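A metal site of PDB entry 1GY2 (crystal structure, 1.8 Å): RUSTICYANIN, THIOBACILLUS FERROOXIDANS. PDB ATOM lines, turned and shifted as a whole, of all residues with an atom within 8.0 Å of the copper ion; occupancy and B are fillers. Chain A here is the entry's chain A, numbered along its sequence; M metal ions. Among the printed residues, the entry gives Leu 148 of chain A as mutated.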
ATOM      1  N   ALA A  44      19.000   8.786 -13.210  1.00  0.00           N
ATOM      2  CA  ALA A  44      17.716   8.286 -12.775  1.00  0.00           C
ATOM      3  C   ALA A  44      16.647   8.644 -13.825  1.00  0.00           C
ATOM      4  O   ALA A  44      16.299   9.823 -14.014  1.00  0.00           O
ATOM      5  CB  ALA A  44      17.353   8.844 -11.436  1.00  0.00           C
ATOM      6  N   VAL A  45      16.113   7.615 -14.482  1.00  0.00           N
ATOM      7  CA  VAL A  45      15.054   7.735 -15.474  1.00  0.00           C
ATOM      8  C   VAL A  45      15.345   8.716 -16.622  1.00  0.00           C
ATOM      9  O   VAL A  45      14.765   9.793 -16.697  1.00  0.00           O
ATOM     10  CB  VAL A  45      13.688   8.059 -14.873  1.00  0.00           C
ATOM     11  CG1 VAL A  45      12.592   7.703 -15.879  1.00  0.00           C
ATOM     12  CG2 VAL A  45      13.462   7.282 -13.586  1.00  0.00           C
ATOM     13  N   PHE A  51       9.917   3.992 -15.807  1.00  0.00           N
ATOM     14  CA  PHE A  51       9.962   4.419 -14.426  1.00  0.00           C
ATOM     15  C   PHE A  51       9.602   3.238 -13.548  1.00  0.00           C
ATOM     16  O   PHE A  51       8.602   2.561 -13.795  1.00  0.00           O
ATOM     17  CB  PHE A  51       8.943   5.508 -14.203  1.00  0.00           C
ATOM     18  CG  PHE A  51       8.777   5.882 -12.770  1.00  0.00           C
ATOM     19  CD1 PHE A  51       7.991   5.152 -11.929  1.00  0.00           C
ATOM     20  CD2 PHE A  51       9.408   6.974 -12.262  1.00  0.00           C
ATOM     21  CE1 PHE A  51       7.863   5.521 -10.622  1.00  0.00           C
ATOM     22  CE2 PHE A  51       9.251   7.321 -10.959  1.00  0.00           C
ATOM     23  CZ  PHE A  51       8.501   6.599 -10.156  1.00  0.00           C
ATOM     24  N   PRO A  52      10.377   2.976 -12.500  1.00  0.00           N
ATOM     25  CA  PRO A  52      11.598   3.694 -12.163  1.00  0.00           C
ATOM     26  C   PRO A  52      12.823   2.868 -12.509  1.00  0.00           C
ATOM     27  O   PRO A  52      12.876   1.662 -12.221  1.00  0.00           O
ATOM     28  CB  PRO A  52      11.480   3.781 -10.653  1.00  0.00           C
ATOM     29  CG  PRO A  52      10.698   2.515 -10.282  1.00  0.00           C
ATOM     30  CD  PRO A  52      10.059   1.948 -11.499  1.00  0.00           C
ATOM     31  N   SER A  53      13.822   3.491 -13.111  1.00  0.00           N
ATOM     32  CA  SER A  53      15.039   2.791 -13.421  1.00  0.00           C
ATOM     33  C   SER A  53      16.236   3.735 -13.440  1.00  0.00           C
ATOM     34  O   SER A  53      16.084   4.947 -13.582  1.00  0.00           O
ATOM     35  CB  SER A  53      14.907   2.121 -14.771  1.00  0.00           C
ATOM     36  OG  SER A  53      14.792   3.075 -15.808  1.00  0.00           O
ATOM     37  N   PHE A  54      17.428   3.168 -13.289  1.00  0.00           N
ATOM     38  CA  PHE A  54      18.658   3.913 -13.506  1.00  0.00           C
ATOM     39  C   PHE A  54      19.231   3.539 -14.881  1.00  0.00           C
ATOM     40  O   PHE A  54      19.217   2.372 -15.228  1.00  0.00           O
ATOM     41  CB  PHE A  54      19.736   3.520 -12.500  1.00  0.00           C
ATOM     42  CG  PHE A  54      19.449   3.957 -11.094  1.00  0.00           C
ATOM     43  CD1 PHE A  54      19.449   5.305 -10.760  1.00  0.00           C
ATOM     44  CD2 PHE A  54      19.218   3.028 -10.110  1.00  0.00           C
ATOM     45  CE1 PHE A  54      19.197   5.713  -9.441  1.00  0.00           C
ATOM     46  CE2 PHE A  54      18.970   3.438  -8.801  1.00  0.00           C
ATOM     47  CZ  PHE A  54      18.961   4.775  -8.472  1.00  0.00           C
ATOM     48  N   PHE A  76      26.327  10.770 -10.586  1.00  0.00           N
ATOM     49  CA  PHE A  76      24.903  10.452 -10.558  1.00  0.00           C
ATOM     50  C   PHE A  76      24.104  11.700 -10.920  1.00  0.00           C
ATOM     51  O   PHE A  76      24.309  12.776 -10.307  1.00  0.00           O
ATOM     52  CB  PHE A  76      24.445   9.958  -9.181  1.00  0.00           C
ATOM     53  CG  PHE A  76      22.958   9.816  -9.067  1.00  0.00           C
ATOM     54  CD1 PHE A  76      22.245   9.041  -9.984  1.00  0.00           C
ATOM     55  CD2 PHE A  76      22.251  10.470  -8.072  1.00  0.00           C
ATOM     56  CE1 PHE A  76      20.880   8.945  -9.913  1.00  0.00           C
ATOM     57  CE2 PHE A  76      20.868  10.350  -7.979  1.00  0.00           C
ATOM     58  CZ  PHE A  76      20.190   9.578  -8.904  1.00  0.00           C
ATOM     59  N   ASN A  78      20.120  13.157 -11.789  1.00  0.00           N
ATOM     60  CA  ASN A  78      18.685  12.863 -11.708  1.00  0.00           C
ATOM     61  C   ASN A  78      17.962  13.581 -12.836  1.00  0.00           C
ATOM     62  O   ASN A  78      17.809  14.783 -12.785  1.00  0.00           O
ATOM     63  CB  ASN A  78      18.119  13.280 -10.357  1.00  0.00           C
ATOM     64  CG  ASN A  78      16.620  13.163 -10.298  1.00  0.00           C
ATOM     65  OD1 ASN A  78      15.947  13.895  -9.538  1.00  0.00           O
ATOM     66  ND2 ASN A  78      16.070  12.259 -11.095  1.00  0.00           N
ATOM     67  N   ASN A  80      14.789  12.768 -13.802  1.00  0.00           N
ATOM     68  CA  ASN A  80      13.382  12.405 -13.730  1.00  0.00           C
ATOM     69  C   ASN A  80      12.515  13.486 -13.094  1.00  0.00           C
ATOM     70  O   ASN A  80      12.585  13.712 -11.893  1.00  0.00           O
ATOM     71  CB  ASN A  80      13.255  11.113 -12.940  1.00  0.00           C
ATOM     72  CG  ASN A  80      11.905  10.438 -13.115  1.00  0.00           C
ATOM     73  OD1 ASN A  80      11.229  10.566 -14.154  1.00  0.00           O
ATOM     74  ND2 ASN A  80      11.504   9.714 -12.104  1.00  0.00           N
ATOM     75  N   PHE A  83      10.795  13.999  -9.031  1.00  0.00           N
ATOM     76  CA  PHE A  83      11.345  13.150  -7.965  1.00  0.00           C
ATOM     77  C   PHE A  83      12.755  13.587  -7.583  1.00  0.00           C
ATOM     78  O   PHE A  83      13.427  14.214  -8.396  1.00  0.00           O
ATOM     79  CB  PHE A  83      11.360  11.683  -8.407  1.00  0.00           C
ATOM     80  CG  PHE A  83       9.996  11.140  -8.699  1.00  0.00           C
ATOM     81  CD1 PHE A  83       9.215  10.606  -7.699  1.00  0.00           C
ATOM     82  CD2 PHE A  83       9.496  11.178  -9.986  1.00  0.00           C
ATOM     83  CE1 PHE A  83       7.960  10.122  -7.975  1.00  0.00           C
ATOM     84  CE2 PHE A  83       8.251  10.674 -10.259  1.00  0.00           C
ATOM     85  CZ  PHE A  83       7.484  10.150  -9.242  1.00  0.00           C
ATOM     86  N   GLY A  84      13.171  13.296  -6.353  1.00  0.00           N
ATOM     87  CA  GLY A  84      14.522  13.618  -5.890  1.00  0.00           C
ATOM     88  C   GLY A  84      15.278  12.323  -5.605  1.00  0.00           C
ATOM     89  O   GLY A  84      15.705  12.082  -4.461  1.00  0.00           O
ATOM     90  N   HIS A  85      15.413  11.460  -6.620  1.00  0.00           N
ATOM     91  CA  HIS A  85      16.005  10.131  -6.434  1.00  0.00           C
ATOM     92  C   HIS A  85      17.414  10.195  -5.866  1.00  0.00           C
ATOM     93  O   HIS A  85      18.141  11.162  -6.116  1.00  0.00           O
ATOM     94  CB  HIS A  85      16.095   9.387  -7.764  1.00  0.00           C
ATOM     95  CG  HIS A  85      14.807   9.228  -8.493  1.00  0.00           C
ATOM     96  ND1 HIS A  85      13.823   8.354  -8.091  1.00  0.00           N
ATOM     97  CD2 HIS A  85      14.344   9.827  -9.613  1.00  0.00           C
ATOM     98  CE1 HIS A  85      12.824   8.386  -8.954  1.00  0.00           C
ATOM     99  NE2 HIS A  85      13.130   9.267  -9.904  1.00  0.00           N
ATOM    100  N   SER A  86      17.794   9.163  -5.117  1.00  0.00           N
ATOM    101  CA  SER A  86      19.145   9.012  -4.568  1.00  0.00           C
ATOM    102  C   SER A  86      19.812   7.845  -5.313  1.00  0.00           C
ATOM    103  O   SER A  86      19.128   7.093  -6.032  1.00  0.00           O
ATOM    104  CB  SER A  86      19.149   8.718  -3.074  1.00  0.00           C
ATOM    105  OG  SER A  86      18.604   7.431  -2.788  1.00  0.00           O
ATOM    106  N   PHE A  87      21.124   7.699  -5.134  1.00  0.00           N
ATOM    107  CA  PHE A  87      21.913   6.619  -5.735  1.00  0.00           C
ATOM    108  C   PHE A  87      22.859   6.172  -4.604  1.00  0.00           C
ATOM    109  O   PHE A  87      23.835   6.876  -4.244  1.00  0.00           O
ATOM    110  CB  PHE A  87      22.652   7.124  -6.981  1.00  0.00           C
ATOM    111  CG  PHE A  87      23.424   6.055  -7.706  1.00  0.00           C
ATOM    112  CD1 PHE A  87      24.691   5.687  -7.272  1.00  0.00           C
ATOM    113  CD2 PHE A  87      22.920   5.462  -8.852  1.00  0.00           C
ATOM    114  CE1 PHE A  87      25.408   4.737  -7.926  1.00  0.00           C
ATOM    115  CE2 PHE A  87      23.666   4.486  -9.520  1.00  0.00           C
ATOM    116  CZ  PHE A  87      24.913   4.132  -9.038  1.00  0.00           C
ATOM    117  N   PHE A 111      19.101  12.505  -1.175  1.00  0.00           N
ATOM    118  CA  PHE A 111      18.083  12.792  -2.183  1.00  0.00           C
ATOM    119  C   PHE A 111      18.579  13.883  -3.151  1.00  0.00           C
ATOM    120  O   PHE A 111      19.169  14.892  -2.746  1.00  0.00           O
ATOM    121  CB  PHE A 111      16.771  13.180  -1.477  1.00  0.00           C
ATOM    122  CG  PHE A 111      16.216  12.067  -0.631  1.00  0.00           C
ATOM    123  CD1 PHE A 111      15.870  10.863  -1.197  1.00  0.00           C
ATOM    124  CD2 PHE A 111      16.104  12.208   0.748  1.00  0.00           C
ATOM    125  CE1 PHE A 111      15.399   9.826  -0.438  1.00  0.00           C
ATOM    126  CE2 PHE A 111      15.617  11.168   1.521  1.00  0.00           C
ATOM    127  CZ  PHE A 111      15.270   9.988   0.926  1.00  0.00           C
ATOM    128  N   SER A 112      18.390  13.686  -4.437  1.00  0.00           N
ATOM    129  CA  SER A 112      18.794  14.698  -5.408  1.00  0.00           C
ATOM    130  C   SER A 112      17.767  15.822  -5.528  1.00  0.00           C
ATOM    131  O   SER A 112      16.609  15.725  -5.077  1.00  0.00           O
ATOM    132  CB  SER A 112      18.971  14.037  -6.779  1.00  0.00           C
ATOM    133  OG  SER A 112      17.750  13.501  -7.220  1.00  0.00           O
ATOM    134  N   VAL A 137      20.908   1.613  -5.299  1.00  0.00           N
ATOM    135  CA  VAL A 137      19.484   1.722  -5.018  1.00  0.00           C
ATOM    136  C   VAL A 137      19.049   3.133  -4.680  1.00  0.00           C
ATOM    137  O   VAL A 137      19.862   3.933  -4.217  1.00  0.00           O
ATOM    138  CB  VAL A 137      19.072   0.845  -3.795  1.00  0.00           C
ATOM    139  CG1 VAL A 137      19.649  -0.530  -3.869  1.00  0.00           C
ATOM    140  CG2 VAL A 137      19.533   1.490  -2.517  1.00  0.00           C
ATOM    141  N   CYS A 138      17.752   3.425  -4.887  1.00  0.00           N
ATOM    142  CA  CYS A 138      17.177   4.684  -4.472  1.00  0.00           C
ATOM    143  C   CYS A 138      16.504   4.477  -3.128  1.00  0.00           C
ATOM    144  O   CYS A 138      15.888   3.443  -2.910  1.00  0.00           O
ATOM    145  CB  CYS A 138      16.156   5.192  -5.472  1.00  0.00           C
ATOM    146  SG  CYS A 138      15.349   6.721  -4.936  1.00  0.00           S
ATOM    147  N   GLN A 139      16.585   5.463  -2.240  1.00  0.00           N
ATOM    148  CA  GLN A 139      15.960   5.385  -0.925  1.00  0.00           C
ATOM    149  C   GLN A 139      14.555   5.959  -0.833  1.00  0.00           C
ATOM    150  O   GLN A 139      13.923   5.846   0.227  1.00  0.00           O
ATOM    151  CB  GLN A 139      16.782   6.145   0.129  1.00  0.00           C
ATOM    152  CG  GLN A 139      18.147   5.654   0.379  1.00  0.00           C
ATOM    153  CD  GLN A 139      18.783   6.419   1.524  1.00  0.00           C
ATOM    154  OE1 GLN A 139      19.498   7.402   1.304  1.00  0.00           O
ATOM    155  NE2 GLN A 139      18.523   5.979   2.746  1.00  0.00           N
ATOM    156  N   ILE A 140      14.049   6.607  -1.877  1.00  0.00           N
ATOM    157  CA  ILE A 140      12.675   7.139  -1.832  1.00  0.00           C
ATOM    158  C   ILE A 140      11.699   5.989  -1.584  1.00  0.00           C
ATOM    159  O   ILE A 140      11.723   5.005  -2.302  1.00  0.00           O
ATOM    160  CB  ILE A 140      12.303   7.843  -3.119  1.00  0.00           C
ATOM    161  CG1 ILE A 140      13.160   9.114  -3.267  1.00  0.00           C
ATOM    162  CG2 ILE A 140      10.801   8.130  -3.157  1.00  0.00           C
ATOM    163  CD1 ILE A 140      12.765   9.927  -4.451  1.00  0.00           C
ATOM    164  N   PRO A 141      10.839   6.092  -0.571  1.00  0.00           N
ATOM    165  CA  PRO A 141       9.915   4.999  -0.242  1.00  0.00           C
ATOM    166  C   PRO A 141       9.188   4.432  -1.427  1.00  0.00           C
ATOM    167  O   PRO A 141       8.580   5.166  -2.218  1.00  0.00           O
ATOM    168  CB  PRO A 141       8.972   5.663   0.751  1.00  0.00           C
ATOM    169  CG  PRO A 141       9.853   6.646   1.458  1.00  0.00           C
ATOM    170  CD  PRO A 141      10.718   7.216   0.377  1.00  0.00           C
ATOM    171  N   GLY A 142       9.272   3.111  -1.564  1.00  0.00           N
ATOM    172  CA  GLY A 142       8.635   2.401  -2.658  1.00  0.00           C
ATOM    173  C   GLY A 142       9.413   2.269  -3.955  1.00  0.00           C
ATOM    174  O   GLY A 142       9.074   1.423  -4.749  1.00  0.00           O
ATOM    175  N   HIS A 143      10.437   3.087  -4.176  1.00  0.00           N
ATOM    176  CA  HIS A 143      11.161   3.059  -5.457  1.00  0.00           C
ATOM    177  C   HIS A 143      11.981   1.791  -5.672  1.00  0.00           C
ATOM    178  O   HIS A 143      11.893   1.185  -6.726  1.00  0.00           O
ATOM    179  CB  HIS A 143      12.016   4.304  -5.652  1.00  0.00           C
ATOM    180  CG  HIS A 143      11.193   5.524  -5.951  1.00  0.00           C
ATOM    181  ND1 HIS A 143      11.743   6.738  -6.299  1.00  0.00           N
ATOM    182  CD2 HIS A 143       9.848   5.701  -5.966  1.00  0.00           C
ATOM    183  CE1 HIS A 143      10.777   7.615  -6.517  1.00  0.00           C
ATOM    184  NE2 HIS A 143       9.613   7.009  -6.321  1.00  0.00           N
ATOM    185  N   ALA A 144      12.785   1.416  -4.682  1.00  0.00           N
ATOM    186  CA  ALA A 144      13.575   0.190  -4.741  1.00  0.00           C
ATOM    187  C   ALA A 144      12.638  -1.033  -4.834  1.00  0.00           C
ATOM    188  O   ALA A 144      12.902  -1.984  -5.563  1.00  0.00           O
ATOM    189  CB  ALA A 144      14.463   0.093  -3.531  1.00  0.00           C
ATOM    190  N   THR A 146       9.888  -1.147  -6.255  1.00  0.00           N
ATOM    191  CA  THR A 146       9.283  -1.217  -7.564  1.00  0.00           C
ATOM    192  C   THR A 146      10.275  -1.225  -8.707  1.00  0.00           C
ATOM    193  O   THR A 146       9.882  -0.942  -9.833  1.00  0.00           O
ATOM    194  CB  THR A 146       8.191  -0.160  -7.783  1.00  0.00           C
ATOM    195  OG1 THR A 146       8.683   1.153  -7.471  1.00  0.00           O
ATOM    196  CG2 THR A 146       7.013  -0.412  -6.821  1.00  0.00           C
ATOM    197  N   LEU A 148      13.770   0.167  -8.781  1.00  0.00           N
ATOM    198  CA  LEU A 148      14.853   1.154  -8.924  1.00  0.00           C
ATOM    199  C   LEU A 148      16.117   0.688  -8.224  1.00  0.00           C
ATOM    200  O   LEU A 148      16.453   1.173  -7.156  1.00  0.00           O
ATOM    201  CB  LEU A 148      14.440   2.539  -8.419  1.00  0.00           C
ATOM    202  CG  LEU A 148      15.417   3.698  -8.752  1.00  0.00           C
ATOM    203  CD1 LEU A 148      15.943   3.659 -10.186  1.00  0.00           C
ATOM    204  CD2 LEU A 148      14.724   5.030  -8.458  1.00  0.00           C
HETATM  205 CU    CU M   1      13.717   7.142  -6.398  1.00  0.00          CU
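Ile 140 touches the copper ion (CD1 to CU, 3.5 Å).
Leu 148 touches the copper ion (CD2 to CU, 3.1 Å).
Within 4 Å of the copper ion: His 85, Cys 138, Ile 140, His 143 and Leu 148.
Along chain A the residues within 4 Å of the copper ion span positions 85 to 148.
The nearest printed residue that does not touch the copper ion is Ser 86 (4.7 Å).
O of His 143 is in hydrogen-bond range of N of Leu 148, at 3.0 Å.
The side-chain hydroxyl (OG1) of Thr 146 lies within hydrogen-bond range of the backbone carbonyl oxygen (O) of His 143, at 3.3 Å.
A ring nitrogen (NE2) of His 85 sits at hydrogen-bond distance from the side-chain amide nitrogen of Asn 80 (2.8 Å).
The backbone carbonyl oxygen (O) of His 85 sits at hydrogen-bond distance from the side-chain hydroxyl (OG) of Ser 112 (2.6 Å).
N of Cys 138 lies within hydrogen-bond range of O of Leu 148.
The side-chain sulfur (SG) of Cys 138 lies close to the backbone NH (N) of Ile 140.
N of Ser 86 lies close to SG of Cys 138.
The copper ion is bound by ND1 of His 143, ND1 of His 85 and SG of Cys 138.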
